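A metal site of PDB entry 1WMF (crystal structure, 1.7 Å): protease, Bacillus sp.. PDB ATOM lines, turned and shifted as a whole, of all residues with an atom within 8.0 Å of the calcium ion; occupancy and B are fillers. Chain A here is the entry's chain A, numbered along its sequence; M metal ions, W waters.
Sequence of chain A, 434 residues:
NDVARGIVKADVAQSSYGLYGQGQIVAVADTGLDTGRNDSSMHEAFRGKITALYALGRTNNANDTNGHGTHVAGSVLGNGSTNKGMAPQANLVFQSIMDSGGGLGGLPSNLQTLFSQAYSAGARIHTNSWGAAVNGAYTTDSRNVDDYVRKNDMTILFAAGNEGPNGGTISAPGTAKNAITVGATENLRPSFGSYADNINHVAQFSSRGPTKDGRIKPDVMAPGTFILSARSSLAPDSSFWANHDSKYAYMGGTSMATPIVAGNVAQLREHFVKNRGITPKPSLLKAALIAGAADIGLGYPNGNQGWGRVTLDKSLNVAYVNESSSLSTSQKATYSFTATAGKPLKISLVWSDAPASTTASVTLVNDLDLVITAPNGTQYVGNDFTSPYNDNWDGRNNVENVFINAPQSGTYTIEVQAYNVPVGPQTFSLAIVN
The backbone carbonyl oxygen (O) of Ser 194 binds the calcium ion (2.2 Å). The calcium ion is bound by water W1 (2.4 Å). The calcium ion is bound by the side-chain carboxylate (OD1) of Asp 197, 2.4 Å away. The calcium ion is bound by OE2 of Glu 186 (2.4 Å). Water W2 is bound to the calcium ion (2.4 Å). The side-chain carboxylate (OE1) of Glu 186 binds the calcium ion. ND1 of His 201 binds the calcium ion.
Of the 15 residues printed, 4 come within 4 Å of the calcium ion. The nearest printed residue that does not touch the calcium ion is Tyr 195 (4.5 Å).
The side-chain carboxylate (OE2) of Glu 186 sits close to the backbone NH (N) of Asn 198 (3.2 Å). The side-chain amide nitrogen (ND2) of Asn 198 is in hydrogen-bond range of a ring nitrogen (NE2) of His 201 (3.1 Å).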
ATOM      1  N   GLU A 186       7.651   8.397   8.005  1.00  0.00           N
ATOM      2  CA  GLU A 186       6.654   8.731   9.026  1.00  0.00           C
ATOM      3  C   GLU A 186       5.484   7.757   9.080  1.00  0.00           C
ATOM      4  O   GLU A 186       4.996   7.281   8.076  1.00  0.00           O
ATOM      5  CB  GLU A 186       6.124  10.145   8.754  1.00  0.00           C
ATOM      6  CG  GLU A 186       7.233  11.185   8.740  1.00  0.00           C
ATOM      7  CD  GLU A 186       6.688  12.610   8.759  1.00  0.00           C
ATOM      8  OE1 GLU A 186       7.498  13.555   8.799  1.00  0.00           O
ATOM      9  OE2 GLU A 186       5.483  12.834   8.445  1.00  0.00           O
ATOM     10  N   ASN A 187       5.030   7.467  10.305  1.00  0.00           N
ATOM     11  CA  ASN A 187       3.751   6.764  10.457  1.00  0.00           C
ATOM     12  C   ASN A 187       2.635   7.735  10.106  1.00  0.00           C
ATOM     13  O   ASN A 187       2.810   8.955  10.123  1.00  0.00           O
ATOM     14  CB  ASN A 187       3.607   6.198  11.865  1.00  0.00           C
ATOM     15  CG  ASN A 187       2.708   4.994  11.989  1.00  0.00           C
ATOM     16  OD1 ASN A 187       2.260   4.428  10.975  1.00  0.00           O
ATOM     17  ND2 ASN A 187       2.421   4.580  13.223  1.00  0.00           N
ATOM     18  N   GLY A 193       0.825  15.471  14.853  1.00  0.00           N
ATOM     19  CA  GLY A 193       1.660  16.501  14.294  1.00  0.00           C
ATOM     20  C   GLY A 193       2.522  16.163  13.111  1.00  0.00           C
ATOM     21  O   GLY A 193       2.378  15.134  12.435  1.00  0.00           O
ATOM     22  N   SER A 194       3.453  17.060  12.787  1.00  0.00           N
ATOM     23  CA  SER A 194       4.190  16.943  11.541  1.00  0.00           C
ATOM     24  C   SER A 194       5.094  15.730  11.466  1.00  0.00           C
ATOM     25  O   SER A 194       5.541  15.360  10.380  1.00  0.00           O
ATOM     26  CB  SER A 194       5.049  18.198  11.296  1.00  0.00           C
ATOM     27  OG  SER A 194       6.106  18.249  12.227  1.00  0.00           O
ATOM     28  N   TYR A 195       5.352  15.111  12.610  1.00  0.00           N
ATOM     29  CA  TYR A 195       6.227  13.936  12.537  1.00  0.00           C
ATOM     30  C   TYR A 195       5.456  12.708  12.095  1.00  0.00           C
ATOM     31  O   TYR A 195       6.096  11.689  11.886  1.00  0.00           O
ATOM     32  CB  TYR A 195       6.878  13.648  13.899  1.00  0.00           C
ATOM     33  CG  TYR A 195       8.217  14.348  14.081  1.00  0.00           C
ATOM     34  CD1 TYR A 195       8.224  15.660  14.560  1.00  0.00           C
ATOM     35  CD2 TYR A 195       9.422  13.750  13.774  1.00  0.00           C
ATOM     36  CE1 TYR A 195       9.418  16.332  14.729  1.00  0.00           C
ATOM     37  CE2 TYR A 195      10.631  14.408  13.953  1.00  0.00           C
ATOM     38  CZ  TYR A 195      10.613  15.707  14.430  1.00  0.00           C
ATOM     39  OH  TYR A 195      11.769  16.420  14.622  1.00  0.00           O
ATOM     40  N   ALA A 196       4.138  12.760  11.988  1.00  0.00           N
ATOM     41  CA  ALA A 196       3.378  11.578  11.583  1.00  0.00           C
ATOM     42  C   ALA A 196       2.231  11.934  10.657  1.00  0.00           C
ATOM     43  O   ALA A 196       1.091  11.457  10.806  1.00  0.00           O
ATOM     44  CB  ALA A 196       2.862  10.810  12.782  1.00  0.00           C
ATOM     45  N   ASP A 197       2.515  12.779   9.652  1.00  0.00           N
ATOM     46  CA  ASP A 197       1.436  13.154   8.747  1.00  0.00           C
ATOM     47  C   ASP A 197       1.652  12.753   7.303  1.00  0.00           C
ATOM     48  O   ASP A 197       0.723  13.015   6.532  1.00  0.00           O
ATOM     49  CB  ASP A 197       1.233  14.672   8.779  1.00  0.00           C
ATOM     50  CG  ASP A 197       2.389  15.514   8.310  1.00  0.00           C
ATOM     51  OD1 ASP A 197       3.476  15.016   7.941  1.00  0.00           O
ATOM     52  OD2 ASP A 197       2.257  16.759   8.309  1.00  0.00           O
ATOM     53  N   ASN A 198       2.767  12.181   6.872  1.00  0.00           N
ATOM     54  CA  ASN A 198       2.942  11.807   5.453  1.00  0.00           C
ATOM     55  C   ASN A 198       3.795  10.559   5.352  1.00  0.00           C
ATOM     56  O   ASN A 198       4.979  10.607   5.665  1.00  0.00           O
ATOM     57  CB  ASN A 198       3.595  12.939   4.650  1.00  0.00           C
ATOM     58  CG  ASN A 198       3.604  12.667   3.160  1.00  0.00           C
ATOM     59  OD1 ASN A 198       3.695  11.512   2.729  1.00  0.00           O
ATOM     60  ND2 ASN A 198       3.507  13.750   2.367  1.00  0.00           N
ATOM     61  N   ILE A 199       3.223   9.434   4.927  1.00  0.00           N
ATOM     62  CA  ILE A 199       3.961   8.180   4.891  1.00  0.00           C
ATOM     63  C   ILE A 199       5.104   8.181   3.877  1.00  0.00           C
ATOM     64  O   ILE A 199       5.880   7.213   3.913  1.00  0.00           O
ATOM     65  CB  ILE A 199       3.042   6.993   4.525  1.00  0.00           C
ATOM     66  CG1 ILE A 199       2.529   6.998   3.085  1.00  0.00           C
ATOM     67  CG2 ILE A 199       1.911   6.906   5.542  1.00  0.00           C
ATOM     68  CD1 ILE A 199       1.773   5.727   2.710  1.00  0.00           C
ATOM     69  N   ASN A 200       5.159   9.196   3.023  1.00  0.00           N
ATOM     70  CA  ASN A 200       6.203   9.370   2.033  1.00  0.00           C
ATOM     71  C   ASN A 200       7.245  10.405   2.440  1.00  0.00           C
ATOM     72  O   ASN A 200       8.077  10.792   1.604  1.00  0.00           O
ATOM     73  CB  ASN A 200       5.583   9.796   0.699  1.00  0.00           C
ATOM     74  CG  ASN A 200       4.886   8.633   0.024  1.00  0.00           C
ATOM     75  OD1 ASN A 200       5.499   7.568  -0.160  1.00  0.00           O
ATOM     76  ND2 ASN A 200       3.616   8.845  -0.305  1.00  0.00           N
ATOM     77  N   HIS A 201       7.221  10.840   3.691  1.00  0.00           N
ATOM     78  CA  HIS A 201       8.207  11.736   4.274  1.00  0.00           C
ATOM     79  C   HIS A 201       9.296  10.942   4.985  1.00  0.00           C
ATOM     80  O   HIS A 201       8.920  10.093   5.799  1.00  0.00           O
ATOM     81  CB  HIS A 201       7.577  12.674   5.292  1.00  0.00           C
ATOM     82  CG  HIS A 201       6.836  13.857   4.783  1.00  0.00           C
ATOM     83  ND1 HIS A 201       6.292  14.831   5.622  1.00  0.00           N
ATOM     84  CD2 HIS A 201       6.507  14.276   3.544  1.00  0.00           C
ATOM     85  CE1 HIS A 201       5.693  15.768   4.940  1.00  0.00           C
ATOM     86  NE2 HIS A 201       5.804  15.451   3.650  1.00  0.00           N
ATOM     87  N   VAL A 202      10.570  11.176   4.738  1.00  0.00           N
ATOM     88  CA  VAL A 202      11.601  10.621   5.613  1.00  0.00           C
ATOM     89  C   VAL A 202      11.528  11.355   6.939  1.00  0.00           C
ATOM     90  O   VAL A 202      11.472  12.608   6.932  1.00  0.00           O
ATOM     91  CB  VAL A 202      13.010  10.808   5.011  1.00  0.00           C
ATOM     92  CG1 VAL A 202      14.036  10.090   5.897  1.00  0.00           C
ATOM     93  CG2 VAL A 202      13.073  10.331   3.571  1.00  0.00           C
ATOM     94  N   ALA A 203      11.533  10.627   8.052  1.00  0.00           N
ATOM     95  CA  ALA A 203      11.548  11.283   9.373  1.00  0.00           C
ATOM     96  C   ALA A 203      12.743  12.227   9.492  1.00  0.00           C
ATOM     97  O   ALA A 203      13.840  11.881   9.033  1.00  0.00           O
ATOM     98  CB  ALA A 203      11.564  10.255  10.494  1.00  0.00           C
ATOM     99  N   GLN A 204      12.557  13.396  10.096  1.00  0.00           N
ATOM    100  CA  GLN A 204      13.623  14.381  10.076  1.00  0.00           C
ATOM    101  C   GLN A 204      14.968  13.866  10.595  1.00  0.00           C
ATOM    102  O   GLN A 204      16.040  14.154  10.054  1.00  0.00           O
ATOM    103  CB  GLN A 204      13.217  15.572  10.960  1.00  0.00           C
ATOM    104  CG  GLN A 204      14.109  16.781  10.704  1.00  0.00           C
ATOM    105  CD  GLN A 204      13.445  18.041  11.217  1.00  0.00           C
ATOM    106  OE1 GLN A 204      13.282  19.038  10.497  1.00  0.00           O
ATOM    107  NE2 GLN A 204      13.057  18.003  12.489  1.00  0.00           N
ATOM    108  N   THR A 225       7.839   6.780  13.220  1.00  0.00           N
ATOM    109  CA  THR A 225       7.493   7.865  14.140  1.00  0.00           C
ATOM    110  C   THR A 225       6.161   7.528  14.829  1.00  0.00           C
ATOM    111  O   THR A 225       5.405   6.838  14.137  1.00  0.00           O
ATOM    112  CB  THR A 225       7.348   9.212  13.432  1.00  0.00           C
ATOM    113  OG1 THR A 225       6.329   9.100  12.434  1.00  0.00           O
ATOM    114  CG2 THR A 225       8.637   9.592  12.713  1.00  0.00           C
HETATM  115 CA    CA M   1       5.833  15.205   8.170  1.00  0.00          CA
HETATM  116  O   HOH W   1       7.678  16.669   8.274  1.00  0.00           O
HETATM  117  O   HOH W   2       4.860  17.351   7.642  1.00  0.00           O
